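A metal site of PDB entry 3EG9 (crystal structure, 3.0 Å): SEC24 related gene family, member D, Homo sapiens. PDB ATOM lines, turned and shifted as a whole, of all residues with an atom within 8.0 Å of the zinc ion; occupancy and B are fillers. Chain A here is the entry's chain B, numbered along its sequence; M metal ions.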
ATOM      1  N   ARG A 100       3.075 -12.951  18.500  1.00  0.00           N
ATOM      2  CA  ARG A 100       2.512 -14.017  19.305  1.00  0.00           C
ATOM      3  C   ARG A 100       2.651 -13.669  20.775  1.00  0.00           C
ATOM      4  O   ARG A 100       3.599 -13.000  21.178  1.00  0.00           O
ATOM      5  CB  ARG A 100       3.237 -15.318  19.036  1.00  0.00           C
ATOM      6  CG  ARG A 100       3.525 -15.524  17.570  1.00  0.00           C
ATOM      7  CD  ARG A 100       4.394 -16.742  17.330  1.00  0.00           C
ATOM      8  NE  ARG A 100       3.872 -17.890  18.055  1.00  0.00           N
ATOM      9  CZ  ARG A 100       4.327 -19.129  17.933  1.00  0.00           C
ATOM     10  NH1 ARG A 100       5.332 -19.384  17.097  1.00  0.00           N
ATOM     11  NH2 ARG A 100       3.786 -20.115  18.645  1.00  0.00           N
ATOM     12  N   CYS A 101       1.697 -14.127  21.560  1.00  0.00           N
ATOM     13  CA  CYS A 101       1.729 -13.914  22.997  1.00  0.00           C
ATOM     14  C   CYS A 101       3.063 -14.495  23.470  1.00  0.00           C
ATOM     15  O   CYS A 101       3.504 -15.524  22.956  1.00  0.00           O
ATOM     16  CB  CYS A 101       0.589 -14.668  23.663  1.00  0.00           C
ATOM     17  SG  CYS A 101       0.853 -14.946  25.401  1.00  0.00           S
ATOM     18  N   ASN A 102       3.715 -13.849  24.432  1.00  0.00           N
ATOM     19  CA  ASN A 102       4.996 -14.363  24.914  1.00  0.00           C
ATOM     20  C   ASN A 102       4.881 -15.578  25.796  1.00  0.00           C
ATOM     21  O   ASN A 102       5.799 -16.394  25.856  1.00  0.00           O
ATOM     22  CB  ASN A 102       5.756 -13.284  25.670  1.00  0.00           C
ATOM     23  CG  ASN A 102       6.420 -12.305  24.745  1.00  0.00           C
ATOM     24  OD1 ASN A 102       5.762 -11.461  24.144  1.00  0.00           O
ATOM     25  ND2 ASN A 102       7.742 -12.426  24.601  1.00  0.00           N
ATOM     26  N   ARG A 103       3.739 -15.719  26.470  1.00  0.00           N
ATOM     27  CA  ARG A 103       3.529 -16.850  27.354  1.00  0.00           C
ATOM     28  C   ARG A 103       3.153 -18.148  26.635  1.00  0.00           C
ATOM     29  O   ARG A 103       3.983 -19.037  26.495  1.00  0.00           O
ATOM     30  CB  ARG A 103       2.468 -16.508  28.416  1.00  0.00           C
ATOM     31  CG  ARG A 103       2.475 -17.460  29.612  1.00  0.00           C
ATOM     32  CD  ARG A 103       1.454 -17.094  30.670  1.00  0.00           C
ATOM     33  NE  ARG A 103       1.764 -15.826  31.338  1.00  0.00           N
ATOM     34  CZ  ARG A 103       0.961 -15.232  32.215  1.00  0.00           C
ATOM     35  NH1 ARG A 103      -0.199 -15.797  32.545  1.00  0.00           N
ATOM     36  NH2 ARG A 103       1.322 -14.080  32.775  1.00  0.00           N
ATOM     37  N   CYS A 104       1.906 -18.245  26.163  1.00  0.00           N
ATOM     38  CA  CYS A 104       1.420 -19.452  25.487  1.00  0.00           C
ATOM     39  C   CYS A 104       1.746 -19.513  23.993  1.00  0.00           C
ATOM     40  O   CYS A 104       1.443 -20.507  23.334  1.00  0.00           O
ATOM     41  CB  CYS A 104      -0.082 -19.567  25.667  1.00  0.00           C
ATOM     42  SG  CYS A 104      -0.939 -18.183  24.965  1.00  0.00           S
ATOM     43  N   LYS A 105       2.339 -18.450  23.477  1.00  0.00           N
ATOM     44  CA  LYS A 105       2.757 -18.361  22.077  1.00  0.00           C
ATOM     45  C   LYS A 105       1.670 -18.407  21.028  1.00  0.00           C
ATOM     46  O   LYS A 105       1.957 -18.691  19.864  1.00  0.00           O
ATOM     47  CB  LYS A 105       3.783 -19.445  21.751  1.00  0.00           C
ATOM     48  CG  LYS A 105       5.073 -19.326  22.521  1.00  0.00           C
ATOM     49  CD  LYS A 105       5.822 -18.059  22.155  1.00  0.00           C
ATOM     50  CE  LYS A 105       7.044 -17.875  23.035  1.00  0.00           C
ATOM     51  NZ  LYS A 105       7.743 -16.582  22.770  1.00  0.00           N
ATOM     52  N   ALA A 106       0.429 -18.127  21.421  1.00  0.00           N
ATOM     53  CA  ALA A 106      -0.667 -18.114  20.464  1.00  0.00           C
ATOM     54  C   ALA A 106      -0.429 -16.998  19.442  1.00  0.00           C
ATOM     55  O   ALA A 106       0.140 -15.951  19.772  1.00  0.00           O
ATOM     56  CB  ALA A 106      -1.977 -17.879  21.187  1.00  0.00           C
ATOM     57  N   TYR A 107      -0.847 -17.209  18.195  1.00  0.00           N
ATOM     58  CA  TYR A 107      -0.649 -16.196  17.166  1.00  0.00           C
ATOM     59  C   TYR A 107      -1.628 -15.025  17.290  1.00  0.00           C
ATOM     60  O   TYR A 107      -2.598 -15.092  18.040  1.00  0.00           O
ATOM     61  CB  TYR A 107      -0.761 -16.833  15.778  1.00  0.00           C
ATOM     62  CG  TYR A 107       0.290 -17.903  15.528  1.00  0.00           C
ATOM     63  CD1 TYR A 107       1.567 -17.564  15.063  1.00  0.00           C
ATOM     64  CD2 TYR A 107       0.038 -19.224  15.847  1.00  0.00           C
ATOM     65  CE1 TYR A 107       2.559 -18.540  14.945  1.00  0.00           C
ATOM     66  CE2 TYR A 107       1.021 -20.197  15.733  1.00  0.00           C
ATOM     67  CZ  TYR A 107       2.274 -19.855  15.291  1.00  0.00           C
ATOM     68  OH  TYR A 107       3.231 -20.836  15.228  1.00  0.00           O
ATOM     69  N   MET A 112      -7.464 -11.500  20.603  1.00  0.00           N
ATOM     70  CA  MET A 112      -6.556 -10.704  21.399  1.00  0.00           C
ATOM     71  C   MET A 112      -7.181  -9.354  21.729  1.00  0.00           C
ATOM     72  O   MET A 112      -7.392  -8.533  20.830  1.00  0.00           O
ATOM     73  CB  MET A 112      -5.223 -10.525  20.660  1.00  0.00           C
ATOM     74  CG  MET A 112      -4.574 -11.860  20.266  1.00  0.00           C
ATOM     75  SD  MET A 112      -4.370 -12.979  21.687  1.00  0.00           S
ATOM     76  CE  MET A 112      -2.738 -13.637  21.397  1.00  0.00           C
ATOM     77  N   TYR A 121      -1.821  -5.573  24.229  1.00  0.00           N
ATOM     78  CA  TYR A 121      -2.958  -6.444  23.948  1.00  0.00           C
ATOM     79  C   TYR A 121      -2.922  -7.589  24.940  1.00  0.00           C
ATOM     80  O   TYR A 121      -1.890  -8.218  25.119  1.00  0.00           O
ATOM     81  CB  TYR A 121      -2.915  -6.981  22.497  1.00  0.00           C
ATOM     82  CG  TYR A 121      -1.931  -8.115  22.219  1.00  0.00           C
ATOM     83  CD1 TYR A 121      -2.183  -9.412  22.683  1.00  0.00           C
ATOM     84  CD2 TYR A 121      -0.755  -7.888  21.501  1.00  0.00           C
ATOM     85  CE1 TYR A 121      -1.281 -10.455  22.433  1.00  0.00           C
ATOM     86  CE2 TYR A 121       0.135  -8.921  21.243  1.00  0.00           C
ATOM     87  CZ  TYR A 121      -0.119 -10.204  21.716  1.00  0.00           C
ATOM     88  OH  TYR A 121       0.795 -11.215  21.497  1.00  0.00           O
ATOM     89  N   GLN A 122      -4.029  -7.824  25.612  1.00  0.00           N
ATOM     90  CA  GLN A 122      -4.044  -8.941  26.541  1.00  0.00           C
ATOM     91  C   GLN A 122      -4.376 -10.178  25.689  1.00  0.00           C
ATOM     92  O   GLN A 122      -5.188 -10.107  24.764  1.00  0.00           O
ATOM     93  CB  GLN A 122      -5.104  -8.728  27.606  1.00  0.00           C
ATOM     94  CG  GLN A 122      -5.121  -9.823  28.646  1.00  0.00           C
ATOM     95  CD  GLN A 122      -6.135  -9.552  29.716  1.00  0.00           C
ATOM     96  OE1 GLN A 122      -6.328 -10.371  30.628  1.00  0.00           O
ATOM     97  NE2 GLN A 122      -6.800  -8.407  29.637  1.00  0.00           N
ATOM     98  N   CYS A 123      -3.747 -11.297  25.988  1.00  0.00           N
ATOM     99  CA  CYS A 123      -4.001 -12.507  25.216  1.00  0.00           C
ATOM    100  C   CYS A 123      -5.256 -13.210  25.705  1.00  0.00           C
ATOM    101  O   CYS A 123      -5.496 -13.299  26.907  1.00  0.00           O
ATOM    102  CB  CYS A 123      -2.814 -13.462  25.327  1.00  0.00           C
ATOM    103  SG  CYS A 123      -3.086 -15.008  24.464  1.00  0.00           S
ATOM    104  N   GLY A 124      -6.037 -13.717  24.759  1.00  0.00           N
ATOM    105  CA  GLY A 124      -7.275 -14.393  25.103  1.00  0.00           C
ATOM    106  C   GLY A 124      -7.145 -15.852  25.496  1.00  0.00           C
ATOM    107  O   GLY A 124      -8.117 -16.464  25.904  1.00  0.00           O
ATOM    108  N   PHE A 125      -5.951 -16.416  25.385  1.00  0.00           N
ATOM    109  CA  PHE A 125      -5.774 -17.823  25.738  1.00  0.00           C
ATOM    110  C   PHE A 125      -5.259 -18.057  27.146  1.00  0.00           C
ATOM    111  O   PHE A 125      -5.633 -19.043  27.793  1.00  0.00           O
ATOM    112  CB  PHE A 125      -4.857 -18.512  24.724  1.00  0.00           C
ATOM    113  CG  PHE A 125      -5.392 -18.511  23.325  1.00  0.00           C
ATOM    114  CD1 PHE A 125      -5.130 -17.447  22.457  1.00  0.00           C
ATOM    115  CD2 PHE A 125      -6.161 -19.573  22.860  1.00  0.00           C
ATOM    116  CE1 PHE A 125      -5.624 -17.439  21.151  1.00  0.00           C
ATOM    117  CE2 PHE A 125      -6.664 -19.572  21.561  1.00  0.00           C
ATOM    118  CZ  PHE A 125      -6.398 -18.506  20.702  1.00  0.00           C
ATOM    119  N   CYS A 126      -4.396 -17.161  27.645  1.00  0.00           N
ATOM    120  CA  CYS A 126      -3.841 -17.305  28.993  1.00  0.00           C
ATOM    121  C   CYS A 126      -3.936 -16.021  29.823  1.00  0.00           C
ATOM    122  O   CYS A 126      -3.450 -15.966  30.951  1.00  0.00           O
ATOM    123  CB  CYS A 126      -2.393 -17.770  28.918  1.00  0.00           C
ATOM    124  SG  CYS A 126      -1.303 -16.675  28.016  1.00  0.00           S
ATOM    125  N   ASN A 127      -4.549 -15.004  29.241  1.00  0.00           N
ATOM    126  CA  ASN A 127      -4.744 -13.719  29.912  1.00  0.00           C
ATOM    127  C   ASN A 127      -3.490 -12.912  30.197  1.00  0.00           C
ATOM    128  O   ASN A 127      -3.528 -11.961  30.977  1.00  0.00           O
ATOM    129  CB  ASN A 127      -5.522 -13.934  31.211  1.00  0.00           C
ATOM    130  CG  ASN A 127      -6.860 -14.628  30.984  1.00  0.00           C
ATOM    131  OD1 ASN A 127      -7.708 -14.130  30.245  1.00  0.00           O
ATOM    132  ND2 ASN A 127      -7.043 -15.782  31.626  1.00  0.00           N
ATOM    133  N   CYS A 128      -2.382 -13.273  29.558  1.00  0.00           N
ATOM    134  CA  CYS A 128      -1.141 -12.529  29.729  1.00  0.00           C
ATOM    135  C   CYS A 128      -1.199 -11.235  28.915  1.00  0.00           C
ATOM    136  O   CYS A 128      -1.764 -11.206  27.826  1.00  0.00           O
ATOM    137  CB  CYS A 128       0.054 -13.341  29.258  1.00  0.00           C
ATOM    138  SG  CYS A 128       1.373 -12.319  28.525  1.00  0.00           S
ATOM    139  N   VAL A 129      -0.614 -10.166  29.451  1.00  0.00           N
ATOM    140  CA  VAL A 129      -0.619  -8.908  28.736  1.00  0.00           C
ATOM    141  C   VAL A 129       0.669  -8.803  27.926  1.00  0.00           C
ATOM    142  O   VAL A 129       1.749  -9.154  28.395  1.00  0.00           O
ATOM    143  CB  VAL A 129      -0.713  -7.715  29.696  1.00  0.00           C
ATOM    144  CG1 VAL A 129      -0.888  -6.416  28.896  1.00  0.00           C
ATOM    145  CG2 VAL A 129      -1.875  -7.912  30.666  1.00  0.00           C
ATOM    146  N   ASN A 130       0.544  -8.344  26.691  1.00  0.00           N
ATOM    147  CA  ASN A 130       1.680  -8.220  25.803  1.00  0.00           C
ATOM    148  C   ASN A 130       1.854  -6.780  25.361  1.00  0.00           C
ATOM    149  O   ASN A 130       0.969  -5.955  25.561  1.00  0.00           O
ATOM    150  CB  ASN A 130       1.478  -9.090  24.554  1.00  0.00           C
ATOM    151  CG  ASN A 130       1.745 -10.558  24.819  1.00  0.00           C
ATOM    152  OD1 ASN A 130       2.839 -11.055  24.554  1.00  0.00           O
ATOM    153  ND2 ASN A 130       0.757 -11.246  25.362  1.00  0.00           N
ATOM    154  N   ARG A 432      -3.274 -25.150  20.282  1.00  0.00           N
ATOM    155  CA  ARG A 432      -3.316 -24.389  21.528  1.00  0.00           C
ATOM    156  C   ARG A 432      -4.747 -24.049  21.933  1.00  0.00           C
ATOM    157  O   ARG A 432      -5.610 -23.852  21.081  1.00  0.00           O
ATOM    158  CB  ARG A 432      -2.508 -23.075  21.397  1.00  0.00           C
ATOM    159  CG  ARG A 432      -1.023 -23.279  21.086  1.00  0.00           C
ATOM    160  CD  ARG A 432      -0.206 -21.977  21.094  1.00  0.00           C
ATOM    161  NE  ARG A 432       1.169 -22.244  20.685  1.00  0.00           N
ATOM    162  CZ  ARG A 432       1.512 -22.568  19.445  1.00  0.00           C
ATOM    163  NH1 ARG A 432       0.572 -22.653  18.505  1.00  0.00           N
ATOM    164  NH2 ARG A 432       2.773 -22.846  19.122  1.00  0.00           N
ATOM    165  N   THR A 433      -4.979 -23.971  23.233  1.00  0.00           N
ATOM    166  CA  THR A 433      -6.309 -23.647  23.731  1.00  0.00           C
ATOM    167  C   THR A 433      -6.223 -22.546  24.787  1.00  0.00           C
ATOM    168  O   THR A 433      -5.130 -22.095  25.144  1.00  0.00           O
ATOM    169  CB  THR A 433      -7.045 -24.893  24.352  1.00  0.00           C
ATOM    170  OG1 THR A 433      -6.344 -25.342  25.515  1.00  0.00           O
ATOM    171  CG2 THR A 433      -7.131 -26.034  23.331  1.00  0.00           C
ATOM    172  N   SER A 434      -7.376 -22.119  25.267  1.00  0.00           N
ATOM    173  CA  SER A 434      -7.458 -21.092  26.281  1.00  0.00           C
ATOM    174  C   SER A 434      -7.344 -21.771  27.643  1.00  0.00           C
ATOM    175  O   SER A 434      -7.364 -22.994  27.732  1.00  0.00           O
ATOM    176  CB  SER A 434      -8.789 -20.351  26.167  1.00  0.00           C
ATOM    177  OG  SER A 434      -9.876 -21.208  26.451  1.00  0.00           O
ATOM    178  N   THR A 435      -7.224 -20.970  28.700  1.00  0.00           N
ATOM    179  CA  THR A 435      -7.117 -21.498  30.057  1.00  0.00           C
ATOM    180  C   THR A 435      -8.242 -22.436  30.478  1.00  0.00           C
ATOM    181  O   THR A 435      -9.413 -22.085  30.359  1.00  0.00           O
ATOM    182  CB  THR A 435      -7.065 -20.344  31.069  1.00  0.00           C
ATOM    183  OG1 THR A 435      -5.989 -19.460  30.737  1.00  0.00           O
ATOM    184  CG2 THR A 435      -6.876 -20.882  32.492  1.00  0.00           C
HETATM  185 ZN    ZN M   1      -1.382 -16.037  25.749  1.00  0.00          ZN
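The side-chain sulfur (SG) of Cys 101 sits close to the backbone NH (N) of Arg 103, at 3.2 Å. N of Cys 101 lies within hydrogen-bond range of O of Ala 106. The backbone NH (N) of Ala 106 sits close to the side-chain sulfur (SG) of Cys 104 (3.8 Å). The side-chain sulfur (SG) of Cys 123 lies close to the backbone NH (N) of Phe 125, at 3.3 Å. The side-chain sulfur (SG) of Cys 123 lies close to the side-chain sulfur (SD) of Met 112, 3.7 Å away. O of Cys 104 lies close to NE of Arg 432, 3.2 Å away. The backbone carbonyl oxygen (O) of Cys 128 lies within hydrogen-bond range of the backbone NH (N) of Cys 123 (2.7 Å). ND2 of Asn 130 lies close to SG of Cys 101 (3.7 Å).
The nearest printed residue that does not touch the zinc ion is Phe 125 (4.4 Å).
The zinc ion is bound by the side-chain sulfur (SG) of Cys 104, the side-chain sulfur (SG) of Cys 126, the side-chain sulfur (SG) of Cys 123 and the side-chain sulfur (SG) of Cys 101. The zinc ion has four donor atoms within binding distance.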
